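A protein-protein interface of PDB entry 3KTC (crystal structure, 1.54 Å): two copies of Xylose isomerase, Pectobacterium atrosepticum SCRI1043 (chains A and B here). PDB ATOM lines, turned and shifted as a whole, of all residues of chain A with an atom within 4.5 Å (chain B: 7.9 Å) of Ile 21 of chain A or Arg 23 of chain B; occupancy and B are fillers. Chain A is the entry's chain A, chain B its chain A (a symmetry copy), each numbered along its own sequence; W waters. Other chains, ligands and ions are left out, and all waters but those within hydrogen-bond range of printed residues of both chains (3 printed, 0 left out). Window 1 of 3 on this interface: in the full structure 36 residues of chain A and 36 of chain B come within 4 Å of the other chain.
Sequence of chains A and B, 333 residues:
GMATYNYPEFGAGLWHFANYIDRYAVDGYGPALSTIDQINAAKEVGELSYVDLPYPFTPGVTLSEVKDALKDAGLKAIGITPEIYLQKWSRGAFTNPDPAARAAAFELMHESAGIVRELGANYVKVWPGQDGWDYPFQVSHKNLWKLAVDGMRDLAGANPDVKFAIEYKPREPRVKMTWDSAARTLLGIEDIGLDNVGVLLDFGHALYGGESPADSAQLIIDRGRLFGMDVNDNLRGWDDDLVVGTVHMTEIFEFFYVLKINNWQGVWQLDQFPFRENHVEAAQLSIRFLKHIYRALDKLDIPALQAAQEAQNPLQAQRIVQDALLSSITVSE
O of Ile 21 of chain A lies close to N of Arg 23 of chain B (3.1 Å).
NZ of Lys 169 of chain A is in hydrogen-bond range of OH of Tyr 24 of chain B.
NH2 of Arg 23 of chain B is in salt-bridge range of OE1 of Glu 172 of chain A.
The guanidinium group (NH2) of Arg 23 of chain B sits at hydrogen-bond distance from the backbone carbonyl oxygen (O) of Asp 239 of chain A (3.1 Å).
The guanidinium group (NH1) of Arg 23 of chain B is in salt-bridge range of the side-chain carboxylate (OD2) of Asp 241 of chain A (2.8 Å).
The side-chain carboxylate of Asp 22 of chain A is in hydrogen-bond range of the side-chain hydroxyl of Tyr 29 of chain A.
OE1 of Glu 172 of chain A lies within salt-bridge range of NZ of Lys 169 of chain A.
NZ of Lys 169 of chain A lies close to OD2 of Asp 239 of chain A, at 3.4 Å.
The backbone NH (N) of Tyr 24 of chain B lies within hydrogen-bond range of the side-chain carboxylate (OD1) of Asp 22 of chain B, at 2.9 Å.
The backbone NH (N) of Ala 25 of chain B lies within hydrogen-bond range of the side-chain carboxylate (OD1) of Asp 22 of chain B (2.8 Å).
The side-chain hydroxyl (OH) of Tyr 29 of chain B lies within hydrogen-bond range of the side-chain carboxylate (OD2) of Asp 22 of chain B (2.4 Å).
Among the printed residues, merely in contact across the chains: Phe 273 of chain A with Arg 23 of chain B, Ile 21 of chain A with Ile 21 of chain B, Asp 22 of chain A with Ile 21 of chain B, Ile 21 of chain A with Asp 22 of chain B, Glu 172 of chain A with Tyr 24 of chain B, Val 26 of chain A with Ile 21 of chain B, Ile 21 of chain A with Val 26 of chain B and Asp 239 of chain A with Tyr 24 of chain B.
Of the printed residues of chain B, Ile 21 of chain A touches Ile 21 (3.3 Å), Asp 22 (3.4 Å), Arg 23 (3.0 Å) and Val 26 (3.6 Å).
Of the printed residues of chain B, Lys 169 of chain A touches Tyr 24.
Of the printed residues of chain B, Val 26 of chain A touches Ile 21 (3.6 Å).
Printed residues of chain A within 4 Å of Ile 21 of chain B: Ile 21 (3.3 Å), Asp 22 (3.4 Å) and Val 26 (3.6 Å).
Printed residues of chain B within 4 Å of Asp 239 of chain A: Arg 23 and Tyr 24.
Of the printed residues of chain A, Asp 22 of chain B touches Ile 21.
Gly 28 of chain B touches none of the printed residues of chain A.
The nearest printed residue of chain A that does not touch Arg 23 of chain B is Phe 275 of chain A (4.1 Å).
The nearest printed residue of chain A that does not touch Tyr 24 of chain B is Phe 273 of chain A (4.6 Å).
Of the 13 printed residues of chain A, 8 touch a printed residue of chain B.
Printed residues of chain A that touch a printed residue of chain B: Ile 21, Asp 22, Val 26, Lys 169, Glu 172, Asp 239, Asp 241 and Phe 273.
Hydrophobic or aromatic side chains of chain A that line the printed part of chain B: Ile 21, Val 26 and Phe 273.
Printed residues of chain B that touch a printed residue of chain A: Ile 21, Asp 22, Arg 23, Tyr 24 and Val 26.
Among the printed residues, Asp or Glu carboxylates within 4 Å of a Lys or Arg side-chain nitrogen of the other chain: Glu 172 of chain A with Arg 23 of chain B, Asp 239 of chain A with Arg 23 of chain B and Asp 241 of chain A with Arg 23 of chain B.
Ile 21 of chain A touches its own counterpart, Ile 21 of chain B.
Ile 21 of chain A touches Asp 22 of chain B, and with the chains exchanged Asp 22 of chain A touches Ile 21 of chain B.
Ile 21 of chain A touches Val 26 of chain B, and with the chains exchanged Val 26 of chain A touches Ile 21 of chain B.
Water W1 bridges the side-chain carboxylate (OE2) of Glu 172 of chain A and the guanidinium group (NE) of Arg 23 of chain B.
Water W2 bridges O of Asp 239 of chain A (2.9 Å) and NH2 of Arg 23 of chain B (3.4 Å).
Water W3 bridges O of Arg 23 of chain B (2.9 Å) and N of Ile 21 of chain A (3.2 Å).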
ATOM      1  N   TYR A  20     -20.979  14.902 -12.693  1.00  0.00           N
ATOM      2  CA  TYR A  20     -21.530  13.629 -12.281  1.00  0.00           C
ATOM      3  C   TYR A  20     -23.031  13.686 -12.071  1.00  0.00           C
ATOM      4  O   TYR A  20     -23.679  14.722 -12.234  1.00  0.00           O
ATOM      5  CB  TYR A  20     -20.811  13.137 -11.005  1.00  0.00           C
ATOM      6  CG  TYR A  20     -19.330  13.302 -11.102  1.00  0.00           C
ATOM      7  CD1 TYR A  20     -18.613  12.685 -12.133  1.00  0.00           C
ATOM      8  CD2 TYR A  20     -18.644  14.111 -10.211  1.00  0.00           C
ATOM      9  CE1 TYR A  20     -17.263  12.867 -12.256  1.00  0.00           C
ATOM     10  CE2 TYR A  20     -17.275  14.303 -10.325  1.00  0.00           C
ATOM     11  CZ  TYR A  20     -16.596  13.685 -11.359  1.00  0.00           C
ATOM     12  OH  TYR A  20     -15.238  13.872 -11.527  1.00  0.00           O
ATOM     13  N   ILE A  21     -23.576  12.549 -11.685  1.00  0.00           N
ATOM     14  CA  ILE A  21     -25.000  12.400 -11.435  1.00  0.00           C
ATOM     15  C   ILE A  21     -25.097  11.282 -10.404  1.00  0.00           C
ATOM     16  O   ILE A  21     -24.239  10.398 -10.368  1.00  0.00           O
ATOM     17  CB  ILE A  21     -25.712  12.060 -12.776  1.00  0.00           C
ATOM     18  CG1 ILE A  21     -27.241  12.180 -12.684  1.00  0.00           C
ATOM     19  CG2 ILE A  21     -25.269  10.687 -13.279  1.00  0.00           C
ATOM     20  CD1 ILE A  21     -27.877  12.170 -14.055  1.00  0.00           C
ATOM     21  N   ASP A  22     -26.115  11.346  -9.543  1.00  0.00           N
ATOM     22  CA  ASP A  22     -26.370  10.287  -8.568  1.00  0.00           C
ATOM     23  C   ASP A  22     -27.875  10.068  -8.456  1.00  0.00           C
ATOM     24  O   ASP A  22     -28.665  10.694  -9.180  1.00  0.00           O
ATOM     25  CB  ASP A  22     -25.652  10.507  -7.222  1.00  0.00           C
ATOM     26  CG  ASP A  22     -26.155  11.688  -6.445  1.00  0.00           C
ATOM     27  OD1 ASP A  22     -27.315  12.103  -6.633  1.00  0.00           O
ATOM     28  OD2 ASP A  22     -25.373  12.197  -5.603  1.00  0.00           O
ATOM     29  N   ALA A  25     -29.478  13.775  -7.005  1.00  0.00           N
ATOM     30  CA  ALA A  25     -29.317  14.883  -7.942  1.00  0.00           C
ATOM     31  C   ALA A  25     -29.360  14.263  -9.338  1.00  0.00           C
ATOM     32  O   ALA A  25     -28.357  14.196 -10.057  1.00  0.00           O
ATOM     33  CB  ALA A  25     -27.973  15.665  -7.698  1.00  0.00           C
ATOM     34  N   VAL A  26     -30.551  13.830  -9.728  1.00  0.00           N
ATOM     35  CA  VAL A  26     -30.740  13.127 -10.986  1.00  0.00           C
ATOM     36  C   VAL A  26     -30.629  14.058 -12.170  1.00  0.00           C
ATOM     37  O   VAL A  26     -30.574  13.593 -13.306  1.00  0.00           O
ATOM     38  CB  VAL A  26     -32.099  12.391 -11.027  1.00  0.00           C
ATOM     39  CG1 VAL A  26     -32.192  11.380  -9.868  1.00  0.00           C
ATOM     40  CG2 VAL A  26     -33.270  13.396 -11.050  1.00  0.00           C
ATOM     41  N   GLY A  28     -28.083  16.123 -12.310  1.00  0.00           N
ATOM     42  CA  GLY A  28     -26.635  16.246 -12.466  1.00  0.00           C
ATOM     43  C   GLY A  28     -26.008  17.291 -11.591  1.00  0.00           C
ATOM     44  O   GLY A  28     -26.684  18.168 -11.128  1.00  0.00           O
ATOM     45  N   TYR A  29     -24.708  17.138 -11.359  1.00  0.00           N
ATOM     46  CA  TYR A  29     -23.871  18.093 -10.633  1.00  0.00           C
ATOM     47  C   TYR A  29     -23.099  18.885 -11.673  1.00  0.00           C
ATOM     48  O   TYR A  29     -21.869  18.814 -11.742  1.00  0.00           O
ATOM     49  CB  TYR A  29     -22.862  17.387  -9.718  1.00  0.00           C
ATOM     50  CG  TYR A  29     -23.457  16.642  -8.538  1.00  0.00           C
ATOM     51  CD1 TYR A  29     -23.973  15.384  -8.693  1.00  0.00           C
ATOM     52  CD2 TYR A  29     -23.503  17.218  -7.270  1.00  0.00           C
ATOM     53  CE1 TYR A  29     -24.527  14.691  -7.599  1.00  0.00           C
ATOM     54  CE2 TYR A  29     -24.044  16.537  -6.170  1.00  0.00           C
ATOM     55  CZ  TYR A  29     -24.565  15.280  -6.350  1.00  0.00           C
ATOM     56  OH  TYR A  29     -25.104  14.597  -5.275  1.00  0.00           O
ATOM     57  N   LYS A 169     -12.569  -3.639  -6.499  1.00  0.00           N
ATOM     58  CA  LYS A 169     -13.324  -2.717  -5.696  1.00  0.00           C
ATOM     59  C   LYS A 169     -14.243  -3.524  -4.795  1.00  0.00           C
ATOM     60  O   LYS A 169     -14.848  -4.455  -5.263  1.00  0.00           O
ATOM     61  CB  LYS A 169     -14.138  -1.767  -6.573  1.00  0.00           C
ATOM     62  CG  LYS A 169     -14.695  -0.567  -5.833  1.00  0.00           C
ATOM     63  CD  LYS A 169     -15.647   0.206  -6.697  1.00  0.00           C
ATOM     64  CE  LYS A 169     -16.178   1.419  -5.978  1.00  0.00           C
ATOM     65  NZ  LYS A 169     -17.219   2.120  -6.791  1.00  0.00           N
ATOM     66  N   GLU A 172     -20.197  -1.249  -5.002  1.00  0.00           N
ATOM     67  CA  GLU A 172     -20.739  -0.035  -5.608  1.00  0.00           C
ATOM     68  C   GLU A 172     -20.474  -0.036  -7.097  1.00  0.00           C
ATOM     69  O   GLU A 172     -19.324   0.101  -7.512  1.00  0.00           O
ATOM     70  CB  GLU A 172     -20.215   1.250  -4.956  1.00  0.00           C
ATOM     71  CG  GLU A 172     -20.858   2.502  -5.529  1.00  0.00           C
ATOM     72  CD  GLU A 172     -20.036   3.765  -5.347  1.00  0.00           C
ATOM     73  OE1 GLU A 172     -18.859   3.716  -4.951  1.00  0.00           O
ATOM     74  OE2 GLU A 172     -20.580   4.834  -5.708  1.00  0.00           O
ATOM     75  N   ASP A 239     -16.193   4.410  -1.154  1.00  0.00           N
ATOM     76  CA  ASP A 239     -15.322   4.961  -2.207  1.00  0.00           C
ATOM     77  C   ASP A 239     -15.616   6.453  -2.373  1.00  0.00           C
ATOM     78  O   ASP A 239     -16.196   6.893  -3.388  1.00  0.00           O
ATOM     79  CB  ASP A 239     -15.574   4.209  -3.512  1.00  0.00           C
ATOM     80  CG  ASP A 239     -14.551   4.517  -4.567  1.00  0.00           C
ATOM     81  OD1 ASP A 239     -13.398   4.845  -4.193  1.00  0.00           O
ATOM     82  OD2 ASP A 239     -14.881   4.421  -5.781  1.00  0.00           O
ATOM     83  N   ASP A 241     -13.764   8.997  -2.984  1.00  0.00           N
ATOM     84  CA  ASP A 241     -13.085   9.609  -4.138  1.00  0.00           C
ATOM     85  C   ASP A 241     -12.768  11.074  -3.907  1.00  0.00           C
ATOM     86  O   ASP A 241     -12.893  11.893  -4.813  1.00  0.00           O
ATOM     87  CB  ASP A 241     -13.907   9.408  -5.412  1.00  0.00           C
ATOM     88  CG  ASP A 241     -13.837   7.995  -5.939  1.00  0.00           C
ATOM     89  OD1 ASP A 241     -12.770   7.354  -5.814  1.00  0.00           O
ATOM     90  OD2 ASP A 241     -14.832   7.548  -6.533  1.00  0.00           O
ATOM     91  N   PHE A 273     -13.451  12.184  -7.790  1.00  0.00           N
ATOM     92  CA  PHE A 273     -14.733  12.727  -8.244  1.00  0.00           C
ATOM     93  C   PHE A 273     -15.053  13.986  -7.450  1.00  0.00           C
ATOM     94  O   PHE A 273     -15.682  13.906  -6.401  1.00  0.00           O
ATOM     95  CB  PHE A 273     -15.863  11.715  -7.988  1.00  0.00           C
ATOM     96  CG  PHE A 273     -15.955  10.581  -9.020  1.00  0.00           C
ATOM     97  CD1 PHE A 273     -14.983   9.615  -9.117  1.00  0.00           C
ATOM     98  CD2 PHE A 273     -17.059  10.475  -9.863  1.00  0.00           C
ATOM     99  CE1 PHE A 273     -15.091   8.578 -10.050  1.00  0.00           C
ATOM    100  CE2 PHE A 273     -17.171   9.453 -10.787  1.00  0.00           C
ATOM    101  CZ  PHE A 273     -16.188   8.508 -10.879  1.00  0.00           C
ATOM    102  N   PHE A 275     -17.268  16.230  -6.966  1.00  0.00           N
ATOM    103  CA  PHE A 275     -18.683  16.505  -7.268  1.00  0.00           C
ATOM    104  C   PHE A 275     -19.068  17.955  -7.240  1.00  0.00           C
ATOM    105  O   PHE A 275     -19.613  18.483  -8.217  1.00  0.00           O
ATOM    106  CB  PHE A 275     -19.611  15.764  -6.280  1.00  0.00           C
ATOM    107  CG  PHE A 275     -19.796  14.314  -6.575  1.00  0.00           C
ATOM    108  CD1 PHE A 275     -18.916  13.379  -6.063  1.00  0.00           C
ATOM    109  CD2 PHE A 275     -20.904  13.883  -7.274  1.00  0.00           C
ATOM    110  CE1 PHE A 275     -19.114  12.009  -6.329  1.00  0.00           C
ATOM    111  CE2 PHE A 275     -21.091  12.537  -7.531  1.00  0.00           C
ATOM    112  CZ  PHE A 275     -20.203  11.627  -7.064  1.00  0.00           C
ATOM    113  N   ILE B  21     -30.885   6.151 -11.257  1.00  0.00           N
ATOM    114  CA  ILE B  21     -29.689   6.529 -11.991  1.00  0.00           C
ATOM    115  C   ILE B  21     -28.607   6.661 -10.926  1.00  0.00           C
ATOM    116  O   ILE B  21     -28.908   6.987  -9.777  1.00  0.00           O
ATOM    117  CB  ILE B  21     -29.965   7.855 -12.753  1.00  0.00           C
ATOM    118  CG1 ILE B  21     -28.881   8.182 -13.793  1.00  0.00           C
ATOM    119  CG2 ILE B  21     -30.179   9.001 -11.764  1.00  0.00           C
ATOM    120  CD1 ILE B  21     -29.330   9.277 -14.732  1.00  0.00           C
ATOM    121  N   ASP B  22     -27.359   6.367 -11.299  1.00  0.00           N
ATOM    122  CA  ASP B  22     -26.222   6.543 -10.396  1.00  0.00           C
ATOM    123  C   ASP B  22     -25.037   7.084 -11.190  1.00  0.00           C
ATOM    124  O   ASP B  22     -25.153   7.364 -12.394  1.00  0.00           O
ATOM    125  CB  ASP B  22     -25.910   5.294  -9.550  1.00  0.00           C
ATOM    126  CG  ASP B  22     -25.417   4.122 -10.347  1.00  0.00           C
ATOM    127  OD1 ASP B  22     -24.861   4.313 -11.447  1.00  0.00           O
ATOM    128  OD2 ASP B  22     -25.566   2.981  -9.843  1.00  0.00           O
ATOM    129  N   ARG B  23     -23.909   7.285 -10.521  1.00  0.00           N
ATOM    130  CA  ARG B  23     -22.767   7.909 -11.175  1.00  0.00           C
ATOM    131  C   ARG B  23     -22.096   7.057 -12.237  1.00  0.00           C
ATOM    132  O   ARG B  23     -21.229   7.561 -12.977  1.00  0.00           O
ATOM    133  CB  ARG B  23     -21.722   8.348 -10.138  1.00  0.00           C
ATOM    134  CG  ARG B  23     -21.028   7.219  -9.351  1.00  0.00           C
ATOM    135  CD  ARG B  23     -19.863   7.822  -8.601  1.00  0.00           C
ATOM    136  NE  ARG B  23     -19.303   6.928  -7.605  1.00  0.00           N
ATOM    137  CZ  ARG B  23     -18.159   7.161  -6.958  1.00  0.00           C
ATOM    138  NH1 ARG B  23     -17.422   8.218  -7.268  1.00  0.00           N
ATOM    139  NH2 ARG B  23     -17.733   6.319  -6.036  1.00  0.00           N
ATOM    140  N   TYR B  24     -22.495   5.788 -12.325  1.00  0.00           N
ATOM    141  CA  TYR B  24     -21.937   4.842 -13.301  1.00  0.00           C
ATOM    142  C   TYR B  24     -22.930   4.578 -14.425  1.00  0.00           C
ATOM    143  O   TYR B  24     -22.629   4.853 -15.600  1.00  0.00           O
ATOM    144  CB  TYR B  24     -21.534   3.550 -12.582  1.00  0.00           C
ATOM    145  CG  TYR B  24     -20.512   3.776 -11.474  1.00  0.00           C
ATOM    146  CD1 TYR B  24     -19.236   4.210 -11.742  1.00  0.00           C
ATOM    147  CD2 TYR B  24     -20.864   3.618 -10.132  1.00  0.00           C
ATOM    148  CE1 TYR B  24     -18.307   4.437 -10.707  1.00  0.00           C
ATOM    149  CE2 TYR B  24     -19.943   3.836  -9.116  1.00  0.00           C
ATOM    150  CZ  TYR B  24     -18.682   4.226  -9.396  1.00  0.00           C
ATOM    151  OH  TYR B  24     -17.774   4.438  -8.364  1.00  0.00           O
ATOM    152  N   ALA B  25     -24.116   4.059 -14.091  1.00  0.00           N
ATOM    153  CA  ALA B  25     -25.177   3.851 -15.072  1.00  0.00           C
ATOM    154  C   ALA B  25     -25.868   5.205 -15.235  1.00  0.00           C
ATOM    155  O   ALA B  25     -27.012   5.413 -14.817  1.00  0.00           O
ATOM    156  CB  ALA B  25     -26.191   2.738 -14.610  1.00  0.00           C
ATOM    157  N   VAL B  26     -25.163   6.124 -15.881  1.00  0.00           N
ATOM    158  CA  VAL B  26     -25.637   7.489 -16.033  1.00  0.00           C
ATOM    159  C   VAL B  26     -26.771   7.582 -17.027  1.00  0.00           C
ATOM    160  O   VAL B  26     -27.407   8.628 -17.127  1.00  0.00           O
ATOM    161  CB  VAL B  26     -24.495   8.442 -16.455  1.00  0.00           C
ATOM    162  CG1 VAL B  26     -23.365   8.417 -15.408  1.00  0.00           C
ATOM    163  CG2 VAL B  26     -24.005   8.120 -17.883  1.00  0.00           C
ATOM    164  N   ASP B  27     -27.001   6.505 -17.785  1.00  0.00           N
ATOM    165  CA  ASP B  27     -28.136   6.408 -18.701  1.00  0.00           C
ATOM    166  C   ASP B  27     -29.352   5.731 -18.066  1.00  0.00           C
ATOM    167  O   ASP B  27     -30.344   5.483 -18.741  1.00  0.00           O
ATOM    168  CB  ASP B  27     -27.747   5.764 -20.047  1.00  0.00           C
ATOM    169  CG  ASP B  27     -27.090   4.393 -19.921  1.00  0.00           C
ATOM    170  OD1 ASP B  27     -26.717   3.974 -18.810  1.00  0.00           O
ATOM    171  OD2 ASP B  27     -26.918   3.741 -20.981  1.00  0.00           O
ATOM    172  N   GLY B  28     -29.261   5.461 -16.767  1.00  0.00           N
ATOM    173  CA  GLY B  28     -30.405   5.034 -15.965  1.00  0.00           C
ATOM    174  C   GLY B  28     -30.589   3.546 -15.897  1.00  0.00           C
ATOM    175  O   GLY B  28     -30.087   2.843 -16.731  1.00  0.00           O
ATOM    176  N   TYR B  29     -31.293   3.103 -14.861  1.00  0.00           N
ATOM    177  CA  TYR B  29     -31.693   1.710 -14.656  1.00  0.00           C
ATOM    178  C   TYR B  29     -33.149   1.603 -15.072  1.00  0.00           C
ATOM    179  O   TYR B  29     -34.026   1.320 -14.252  1.00  0.00           O
ATOM    180  CB  TYR B  29     -31.581   1.295 -13.184  1.00  0.00           C
ATOM    181  CG  TYR B  29     -30.170   1.224 -12.629  1.00  0.00           C
ATOM    182  CD1 TYR B  29     -29.528   2.357 -12.205  1.00  0.00           C
ATOM    183  CD2 TYR B  29     -29.489   0.012 -12.544  1.00  0.00           C
ATOM    184  CE1 TYR B  29     -28.217   2.293 -11.691  1.00  0.00           C
ATOM    185  CE2 TYR B  29     -28.186  -0.067 -12.025  1.00  0.00           C
ATOM    186  CZ  TYR B  29     -27.558   1.082 -11.615  1.00  0.00           C
ATOM    187  OH  TYR B  29     -26.273   1.020 -11.105  1.00  0.00           O
HETATM  188  O   HOH W   1     -20.744   7.252  -4.458  1.00  0.00           O
HETATM  189  O   HOH W   2     -18.552   8.586  -3.658  1.00  0.00           O
HETATM  190  O   HOH W   3     -21.536  10.486 -13.089  1.00  0.00           O
